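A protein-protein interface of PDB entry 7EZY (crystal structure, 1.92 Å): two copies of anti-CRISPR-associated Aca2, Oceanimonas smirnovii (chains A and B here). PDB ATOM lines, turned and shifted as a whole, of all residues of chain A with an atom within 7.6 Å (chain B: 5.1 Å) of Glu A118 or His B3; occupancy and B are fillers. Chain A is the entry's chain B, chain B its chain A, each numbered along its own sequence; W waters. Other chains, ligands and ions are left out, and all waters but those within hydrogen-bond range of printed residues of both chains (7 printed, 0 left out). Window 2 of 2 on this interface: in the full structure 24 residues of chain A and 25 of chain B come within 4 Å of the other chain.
No position is printed for both chains. Of the 11 pairs that touch across the chains among the printed residues, none has its exchanged pair printed and touching as well.
Of the 13 printed residues of chain B, 6 touch a printed residue of chain A. Printed residues of chain A that touch a printed residue of chain B: Phe A79, Arg A81, Leu A116, Val A117 and Glu A118. Hydrophobic or aromatic side chains of chain A within 4 Å of the printed part of chain B: Phe A79 and Leu A116.
Glu A118 touches two residues of chain B. Of chain A, only Glu A118 comes within 4 Å of His B3. Printed residues of chain A within 4 Å of Ser B37: Arg A81. Printed residues of chain A within 4 Å of Ala B8: Phe A79 (3.5 Å) and Leu A116 (3.6 Å). Of the printed residues of chain A, Gln B7 touches Phe A79 and Arg A81. Trp B35 touches none of the printed residues of chain A. The nearest residue of chain A that does not touch His B3 is Arg A81 (4.2 Å). The nearest printed residue of chain B that does not touch Arg A81 is His B3 (4.2 Å).
Water W6 bridges the side-chain carboxylate of Glu B5 and the backbone NH of Leu A116. Water W7 bridges the side-chain amide oxygen (OE1) of Gln B7 and the backbone carbonyl oxygen (O) of Arg A81. Water W1 bridges OH of Tyr B4 (2.7 Å) and O of Leu A116 (2.8 Å). Water W2 bridges the backbone NH of Glu A118 and the side-chain hydroxyl of Tyr B4. Water W3 bridges OE1 of Glu A118 and NE2 of His B3. Water W4 lies within hydrogen-bond range of the guanidinium group (NH1) of Arg A81 (2.9 Å) and the side-chain amide nitrogen (NE2) of Gln B7 (3.0 Å).
Among the printed residues, pairs that only touch across the chains: Phe A79 with Tyr B4 (3.9 Å), Phe A79 with Gln B7 (3.5 Å), Phe A79 with Ala B8 (3.5 Å), Arg A81 with Gln B7 (3.7 Å), Arg A81 with Glu B36 (3.7 Å), Arg A81 with Ser B37 (3.8 Å), Leu A116 with Tyr B4 (3.5 Å), Leu A116 with Ala B8 (3.6 Å), Val A117 with Tyr B4 (3.8 Å), Glu A118 with His B3 (3.6 Å) and Glu A118 with Tyr B4 (3.9 Å).
The backbone NH (N) of Phe A79 sits at hydrogen-bond distance from the backbone carbonyl oxygen (O) of Val A117, 3.0 Å away. The backbone NH (N) of Val A117 sits at hydrogen-bond distance from the backbone carbonyl oxygen (O) of Leu A77 (2.9 Å). The side-chain amide nitrogen (NE2) of Gln B7 is in hydrogen-bond range of the side-chain carboxylate (OE1) of Glu B36 (3.1 Å). OD2 of Asp A85 is in hydrogen-bond range of N of Arg A81, at 3.5 Å.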
ATOM      1  N   LEU A  77     -19.340   8.260 -22.202  1.00  0.00           N
ATOM      2  CA  LEU A  77     -17.978   8.112 -21.702  1.00  0.00           C
ATOM      3  C   LEU A  77     -18.018   8.012 -20.193  1.00  0.00           C
ATOM      4  O   LEU A  77     -18.755   8.751 -19.538  1.00  0.00           O
ATOM      5  CB  LEU A  77     -17.070   9.304 -22.082  1.00  0.00           C
ATOM      6  CG  LEU A  77     -16.705   9.458 -23.558  1.00  0.00           C
ATOM      7  CD1 LEU A  77     -15.567  10.468 -23.729  1.00  0.00           C
ATOM      8  CD2 LEU A  77     -16.344   8.139 -24.152  1.00  0.00           C
ATOM      9  N   ASN A  78     -17.186   7.122 -19.661  1.00  0.00           N
ATOM     10  CA  ASN A  78     -17.003   7.022 -18.224  1.00  0.00           C
ATOM     11  C   ASN A  78     -16.231   8.230 -17.739  1.00  0.00           C
ATOM     12  O   ASN A  78     -15.200   8.587 -18.318  1.00  0.00           O
ATOM     13  CB  ASN A  78     -16.214   5.775 -17.850  1.00  0.00           C
ATOM     14  CG  ASN A  78     -17.014   4.513 -18.001  1.00  0.00           C
ATOM     15  OD1 ASN A  78     -18.239   4.540 -17.909  1.00  0.00           O
ATOM     16  ND2 ASN A  78     -16.319   3.389 -18.191  1.00  0.00           N
ATOM     17  N   PHE A  79     -16.730   8.853 -16.695  1.00  0.00           N
ATOM     18  CA  PHE A  79     -15.978   9.850 -15.963  1.00  0.00           C
ATOM     19  C   PHE A  79     -15.644   9.252 -14.602  1.00  0.00           C
ATOM     20  O   PHE A  79     -16.528   9.117 -13.745  1.00  0.00           O
ATOM     21  CB  PHE A  79     -16.756  11.155 -15.816  1.00  0.00           C
ATOM     22  CG  PHE A  79     -15.897  12.260 -15.298  1.00  0.00           C
ATOM     23  CD1 PHE A  79     -15.122  13.010 -16.180  1.00  0.00           C
ATOM     24  CD2 PHE A  79     -15.791  12.499 -13.928  1.00  0.00           C
ATOM     25  CE1 PHE A  79     -14.256  14.032 -15.707  1.00  0.00           C
ATOM     26  CE2 PHE A  79     -14.936  13.510 -13.449  1.00  0.00           C
ATOM     27  CZ  PHE A  79     -14.171  14.266 -14.347  1.00  0.00           C
ATOM     28  N   TYR A  80     -14.376   8.896 -14.403  1.00  0.00           N
ATOM     29  CA  TYR A  80     -13.937   8.230 -13.175  1.00  0.00           C
ATOM     30  C   TYR A  80     -13.667   9.261 -12.087  1.00  0.00           C
ATOM     31  O   TYR A  80     -12.685  10.015 -12.165  1.00  0.00           O
ATOM     32  CB  TYR A  80     -12.677   7.410 -13.447  1.00  0.00           C
ATOM     33  CG  TYR A  80     -12.827   6.420 -14.583  1.00  0.00           C
ATOM     34  CD1 TYR A  80     -13.713   5.350 -14.465  1.00  0.00           C
ATOM     35  CD2 TYR A  80     -12.093   6.551 -15.762  1.00  0.00           C
ATOM     36  CE1 TYR A  80     -13.875   4.412 -15.506  1.00  0.00           C
ATOM     37  CE2 TYR A  80     -12.241   5.617 -16.814  1.00  0.00           C
ATOM     38  CZ  TYR A  80     -13.136   4.542 -16.665  1.00  0.00           C
ATOM     39  OH  TYR A  80     -13.296   3.602 -17.672  1.00  0.00           O
ATOM     40  N   ARG A  81     -14.496   9.259 -11.044  1.00  0.00           N
ATOM     41  CA  ARG A  81     -14.288  10.196  -9.944  1.00  0.00           C
ATOM     42  C   ARG A  81     -13.001   9.896  -9.184  1.00  0.00           C
ATOM     43  O   ARG A  81     -12.290  10.819  -8.763  1.00  0.00           O
ATOM     44  CB  ARG A  81     -15.486  10.179  -8.992  1.00  0.00           C
ATOM     45  CG  ARG A  81     -15.438  11.235  -7.881  1.00  0.00           C
ATOM     46  CD  ARG A  81     -16.626  11.144  -6.920  1.00  0.00           C
ATOM     47  NE  ARG A  81     -16.485  10.069  -5.939  1.00  0.00           N
ATOM     48  CZ  ARG A  81     -15.805  10.202  -4.809  1.00  0.00           C
ATOM     49  NH1 ARG A  81     -15.180  11.326  -4.513  1.00  0.00           N
ATOM     50  NH2 ARG A  81     -15.773   9.192  -3.938  1.00  0.00           N
ATOM     51  N   ASP A  85     -12.157   3.898  -9.203  1.00  0.00           N
ATOM     52  CA  ASP A  85     -13.091   3.711 -10.313  1.00  0.00           C
ATOM     53  C   ASP A  85     -12.339   3.396 -11.613  1.00  0.00           C
ATOM     54  O   ASP A  85     -12.666   2.438 -12.361  1.00  0.00           O
ATOM     55  CB  ASP A  85     -13.951   4.981 -10.479  1.00  0.00           C
ATOM     56  CG  ASP A  85     -14.778   5.337  -9.225  1.00  0.00           C
ATOM     57  OD1 ASP A  85     -15.356   4.428  -8.558  1.00  0.00           O
ATOM     58  OD2 ASP A  85     -14.888   6.556  -8.927  1.00  0.00           O
ATOM     59  N   VAL A  89     -12.108  -0.430 -13.897  1.00  0.00           N
ATOM     60  CA  VAL A  89     -12.302  -0.712 -15.326  1.00  0.00           C
ATOM     61  C   VAL A  89     -11.016  -1.198 -16.000  1.00  0.00           C
ATOM     62  O   VAL A  89     -11.022  -2.183 -16.749  1.00  0.00           O
ATOM     63  CB  VAL A  89     -12.897   0.504 -16.052  1.00  0.00           C
ATOM     64  CG1 VAL A  89     -12.877   0.290 -17.546  1.00  0.00           C
ATOM     65  CG2 VAL A  89     -14.329   0.687 -15.606  1.00  0.00           C
ATOM     66  N   LEU A 116     -21.923  11.767 -20.241  1.00  0.00           N
ATOM     67  CA  LEU A 116     -21.057  11.163 -19.245  1.00  0.00           C
ATOM     68  C   LEU A 116     -21.876  10.163 -18.442  1.00  0.00           C
ATOM     69  O   LEU A 116     -23.079  10.346 -18.236  1.00  0.00           O
ATOM     70  CB  LEU A 116     -20.491  12.230 -18.313  1.00  0.00           C
ATOM     71  CG  LEU A 116     -19.484  13.190 -18.941  1.00  0.00           C
ATOM     72  CD1 LEU A 116     -18.971  14.192 -17.869  1.00  0.00           C
ATOM     73  CD2 LEU A 116     -18.326  12.455 -19.678  1.00  0.00           C
ATOM     74  N   VAL A 117     -21.216   9.097 -18.000  1.00  0.00           N
ATOM     75  CA  VAL A 117     -21.821   8.131 -17.093  1.00  0.00           C
ATOM     76  C   VAL A 117     -20.754   7.794 -16.061  1.00  0.00           C
ATOM     77  O   VAL A 117     -19.564   8.014 -16.291  1.00  0.00           O
ATOM     78  CB  VAL A 117     -22.289   6.871 -17.847  1.00  0.00           C
ATOM     79  CG1 VAL A 117     -23.499   7.202 -18.715  1.00  0.00           C
ATOM     80  CG2 VAL A 117     -21.154   6.303 -18.684  1.00  0.00           C
ATOM     81  N   GLU A 118     -21.165   7.273 -14.898  1.00  0.00           N
ATOM     82  CA  GLU A 118     -20.106   6.767 -14.024  1.00  0.00           C
ATOM     83  C   GLU A 118     -19.698   5.344 -14.377  1.00  0.00           C
ATOM     84  O   GLU A 118     -18.577   4.938 -14.039  1.00  0.00           O
ATOM     85  CB  GLU A 118     -20.453   6.887 -12.534  1.00  0.00           C
ATOM     86  CG  GLU A 118     -21.825   6.504 -12.110  1.00  0.00           C
ATOM     87  CD  GLU A 118     -22.106   6.819 -10.636  1.00  0.00           C
ATOM     88  OE1 GLU A 118     -21.166   6.889  -9.803  1.00  0.00           O
ATOM     89  OE2 GLU A 118     -23.295   7.041 -10.316  1.00  0.00           O
ATOM     90  N   GLN A 119     -20.569   4.582 -15.048  1.00  0.00           N
ATOM     91  CA  GLN A 119     -20.247   3.210 -15.422  1.00  0.00           C
ATOM     92  C   GLN A 119     -20.909   2.880 -16.749  1.00  0.00           C
ATOM     93  O   GLN A 119     -21.970   3.414 -17.085  1.00  0.00           O
ATOM     94  CB  GLN A 119     -20.698   2.164 -14.384  1.00  0.00           C
ATOM     95  CG  GLN A 119     -20.730   2.640 -12.949  1.00  0.00           C
ATOM     96  CD  GLN A 119     -20.820   1.500 -11.970  1.00  0.00           C
ATOM     97  OE1 GLN A 119     -19.992   1.389 -11.051  1.00  0.00           O
ATOM     98  NE2 GLN A 119     -21.796   0.612 -12.180  1.00  0.00           N
ATOM     99  N   GLY A 120     -20.295   1.961 -17.476  1.00  0.00           N
ATOM    100  CA  GLY A 120     -20.898   1.473 -18.693  1.00  0.00           C
ATOM    101  C   GLY A 120     -20.548   2.246 -19.935  1.00  0.00           C
ATOM    102  O   GLY A 120     -21.118   1.965 -21.000  1.00  0.00           O
ATOM    103  N   GLY A 121     -19.619   3.198 -19.842  1.00  0.00           N
ATOM    104  CA  GLY A 121     -19.311   4.027 -20.987  1.00  0.00           C
ATOM    105  C   GLY A 121     -18.608   3.238 -22.078  1.00  0.00           C
ATOM    106  O   GLY A 121     -18.038   2.165 -21.853  1.00  0.00           O
ATOM    107  N   MET B   1     -28.373  18.033 -12.763  1.00  0.00           N
ATOM    108  CA  MET B   1     -27.020  17.720 -13.194  1.00  0.00           C
ATOM    109  C   MET B   1     -26.425  16.765 -12.155  1.00  0.00           C
ATOM    110  O   MET B   1     -26.623  16.971 -10.957  1.00  0.00           O
ATOM    111  CB  MET B   1     -26.183  19.001 -13.353  1.00  0.00           C
ATOM    112  CG  MET B   1     -24.651  18.818 -13.342  1.00  0.00           C
ATOM    113  SD  MET B   1     -23.765  20.401 -13.333  1.00  0.00           S
ATOM    114  CE  MET B   1     -24.038  20.960 -15.026  1.00  0.00           C
ATOM    115  N   THR B   2     -25.733  15.723 -12.623  1.00  0.00           N
ATOM    116  CA  THR B   2     -25.177  14.701 -11.742  1.00  0.00           C
ATOM    117  C   THR B   2     -23.876  15.178 -11.099  1.00  0.00           C
ATOM    118  O   THR B   2     -23.302  16.203 -11.472  1.00  0.00           O
ATOM    119  CB  THR B   2     -24.847  13.412 -12.488  1.00  0.00           C
ATOM    120  OG1 THR B   2     -23.852  13.669 -13.495  1.00  0.00           O
ATOM    121  CG2 THR B   2     -26.117  12.875 -13.151  1.00  0.00           C
ATOM    122  N   HIS B   3     -23.396  14.390 -10.131  1.00  0.00           N
ATOM    123  CA  HIS B   3     -22.177  14.761  -9.423  1.00  0.00           C
ATOM    124  C   HIS B   3     -20.952  14.746 -10.342  1.00  0.00           C
ATOM    125  O   HIS B   3     -20.103  15.642 -10.258  1.00  0.00           O
ATOM    126  CB  HIS B   3     -22.011  13.861  -8.184  1.00  0.00           C
ATOM    127  CG  HIS B   3     -21.635  12.432  -8.476  1.00  0.00           C
ATOM    128  ND1 HIS B   3     -22.576  11.426  -8.572  1.00  0.00           N
ATOM    129  CD2 HIS B   3     -20.428  11.820  -8.577  1.00  0.00           C
ATOM    130  CE1 HIS B   3     -21.971  10.269  -8.781  1.00  0.00           C
ATOM    131  NE2 HIS B   3     -20.665  10.479  -8.788  1.00  0.00           N
ATOM    132  N   TYR B   4     -20.860  13.779 -11.254  1.00  0.00           N
ATOM    133  CA  TYR B   4     -19.700  13.714 -12.138  1.00  0.00           C
ATOM    134  C   TYR B   4     -19.804  14.704 -13.307  1.00  0.00           C
ATOM    135  O   TYR B   4     -18.773  15.197 -13.772  1.00  0.00           O
ATOM    136  CB  TYR B   4     -19.491  12.280 -12.656  1.00  0.00           C
ATOM    137  CG  TYR B   4     -20.783  11.623 -13.127  1.00  0.00           C
ATOM    138  CD1 TYR B   4     -21.595  10.908 -12.233  1.00  0.00           C
ATOM    139  CD2 TYR B   4     -21.201  11.730 -14.454  1.00  0.00           C
ATOM    140  CE1 TYR B   4     -22.788  10.301 -12.670  1.00  0.00           C
ATOM    141  CE2 TYR B   4     -22.393  11.149 -14.889  1.00  0.00           C
ATOM    142  CZ  TYR B   4     -23.172  10.433 -13.993  1.00  0.00           C
ATOM    143  OH  TYR B   4     -24.336   9.850 -14.429  1.00  0.00           O
ATOM    144  N   GLU B   5     -21.016  15.033 -13.770  1.00  0.00           N
ATOM    145  CA  GLU B   5     -21.177  16.155 -14.713  1.00  0.00           C
ATOM    146  C   GLU B   5     -20.690  17.465 -14.096  1.00  0.00           C
ATOM    147  O   GLU B   5     -19.935  18.243 -14.724  1.00  0.00           O
ATOM    148  CB  GLU B   5     -22.648  16.294 -15.141  1.00  0.00           C
ATOM    149  CG  GLU B   5     -23.065  15.246 -16.179  1.00  0.00           C
ATOM    150  CD  GLU B   5     -24.577  15.154 -16.353  1.00  0.00           C
ATOM    151  OE1 GLU B   5     -25.315  15.858 -15.628  1.00  0.00           O
ATOM    152  OE2 GLU B   5     -25.012  14.383 -17.224  1.00  0.00           O
ATOM    153  N   LEU B   6     -21.134  17.734 -12.863  1.00  0.00           N
ATOM    154  CA  LEU B   6     -20.684  18.926 -12.156  1.00  0.00           C
ATOM    155  C   LEU B   6     -19.164  18.938 -12.020  1.00  0.00           C
ATOM    156  O   LEU B   6     -18.522  19.937 -12.347  1.00  0.00           O
ATOM    157  CB  LEU B   6     -21.335  19.000 -10.783  1.00  0.00           C
ATOM    158  CG  LEU B   6     -20.846  20.162  -9.918  1.00  0.00           C
ATOM    159  CD1 LEU B   6     -21.342  21.475 -10.527  1.00  0.00           C
ATOM    160  CD2 LEU B   6     -21.303  20.019  -8.467  1.00  0.00           C
ATOM    161  N   GLN B   7     -18.570  17.831 -11.543  1.00  0.00           N
ATOM    162  CA  GLN B   7     -17.113  17.797 -11.362  1.00  0.00           C
ATOM    163  C   GLN B   7     -16.367  17.955 -12.679  1.00  0.00           C
ATOM    164  O   GLN B   7     -15.356  18.668 -12.741  1.00  0.00           O
ATOM    165  CB  GLN B   7     -16.671  16.486 -10.706  1.00  0.00           C
ATOM    166  CG  GLN B   7     -15.192  16.472 -10.366  1.00  0.00           C
ATOM    167  CD  GLN B   7     -14.814  15.292  -9.498  1.00  0.00           C
ATOM    168  OE1 GLN B   7     -14.683  14.165  -9.975  1.00  0.00           O
ATOM    169  NE2 GLN B   7     -14.669  15.543  -8.215  1.00  0.00           N
ATOM    170  N   ALA B   8     -16.813  17.260 -13.729  1.00  0.00           N
ATOM    171  CA  ALA B   8     -16.121  17.336 -15.001  1.00  0.00           C
ATOM    172  C   ALA B   8     -16.065  18.777 -15.489  1.00  0.00           C
ATOM    173  O   ALA B   8     -14.998  19.268 -15.893  1.00  0.00           O
ATOM    174  CB  ALA B   8     -16.815  16.420 -16.019  1.00  0.00           C
ATOM    175  N   TRP B  35     -21.579  17.682  -3.326  1.00  0.00           N
ATOM    176  CA  TRP B  35     -22.196  17.801  -4.651  1.00  0.00           C
ATOM    177  C   TRP B  35     -21.388  17.051  -5.709  1.00  0.00           C
ATOM    178  O   TRP B  35     -21.965  16.474  -6.641  1.00  0.00           O
ATOM    179  CB  TRP B  35     -22.336  19.270  -5.068  1.00  0.00           C
ATOM    180  CG  TRP B  35     -23.259  20.084  -4.196  1.00  0.00           C
ATOM    181  CD1 TRP B  35     -24.210  19.609  -3.331  1.00  0.00           C
ATOM    182  CD2 TRP B  35     -23.323  21.522  -4.112  1.00  0.00           C
ATOM    183  NE1 TRP B  35     -24.847  20.660  -2.710  1.00  0.00           N
ATOM    184  CE2 TRP B  35     -24.319  21.843  -3.166  1.00  0.00           C
ATOM    185  CE3 TRP B  35     -22.618  22.563  -4.731  1.00  0.00           C
ATOM    186  CZ2 TRP B  35     -24.643  23.168  -2.829  1.00  0.00           C
ATOM    187  CZ3 TRP B  35     -22.930  23.877  -4.391  1.00  0.00           C
ATOM    188  CH2 TRP B  35     -23.943  24.168  -3.451  1.00  0.00           C
ATOM    189  N   GLU B  36     -20.049  17.042  -5.584  1.00  0.00           N
ATOM    190  CA  GLU B  36     -19.212  16.385  -6.591  1.00  0.00           C
ATOM    191  C   GLU B  36     -19.076  14.875  -6.378  1.00  0.00           C
ATOM    192  O   GLU B  36     -18.667  14.163  -7.303  1.00  0.00           O
ATOM    193  CB  GLU B  36     -17.827  17.048  -6.648  1.00  0.00           C
ATOM    194  CG  GLU B  36     -17.879  18.431  -7.329  1.00  0.00           C
ATOM    195  CD  GLU B  36     -16.518  18.944  -7.805  1.00  0.00           C
ATOM    196  OE1 GLU B  36     -15.483  18.376  -7.402  1.00  0.00           O
ATOM    197  OE2 GLU B  36     -16.492  19.936  -8.576  1.00  0.00           O
ATOM    198  N   SER B  37     -19.414  14.365  -5.195  1.00  0.00           N
ATOM    199  CA  SER B  37     -19.352  12.926  -4.967  1.00  0.00           C
ATOM    200  C   SER B  37     -20.720  12.248  -4.996  1.00  0.00           C
ATOM    201  O   SER B  37     -20.776  11.014  -4.994  1.00  0.00           O
ATOM    202  CB  SER B  37     -18.645  12.622  -3.634  1.00  0.00           C
ATOM    203  OG  SER B  37     -19.439  13.052  -2.549  1.00  0.00           O
ATOM    204  N   GLY B  38     -21.812  13.001  -5.062  1.00  0.00           N
ATOM    205  CA  GLY B  38     -23.130  12.393  -5.099  1.00  0.00           C
ATOM    206  C   GLY B  38     -23.791  12.244  -3.747  1.00  0.00           C
ATOM    207  O   GLY B  38     -24.905  11.714  -3.671  1.00  0.00           O
ATOM    208  N   VAL B  42     -27.020  18.143  -6.576  1.00  0.00           N
ATOM    209  CA  VAL B  42     -26.528  19.417  -7.100  1.00  0.00           C
ATOM    210  C   VAL B  42     -27.695  20.387  -7.243  1.00  0.00           C
ATOM    211  O   VAL B  42     -28.612  20.120  -8.031  1.00  0.00           O
ATOM    212  CB  VAL B  42     -25.850  19.233  -8.465  1.00  0.00           C
ATOM    213  CG1 VAL B  42     -25.373  20.573  -9.008  1.00  0.00           C
ATOM    214  CG2 VAL B  42     -24.689  18.246  -8.365  1.00  0.00           C
HETATM  215  O   HOH W   1     -25.481  10.164 -16.811  1.00  0.00           O
HETATM  216  O   HOH W   2     -23.789   6.736 -14.555  1.00  0.00           O
HETATM  217  O   HOH W   3     -18.794   8.395  -9.330  1.00  0.00           O
HETATM  218  O   HOH W   4     -14.585  13.885  -5.769  1.00  0.00           O
HETATM  219  O   HOH W   5     -19.188   8.779  -5.377  1.00  0.00           O
HETATM  220  O   HOH W   6     -24.167  13.289 -19.286  1.00  0.00           O
HETATM  221  O   HOH W   7     -12.293  13.356  -9.550  1.00  0.00           O
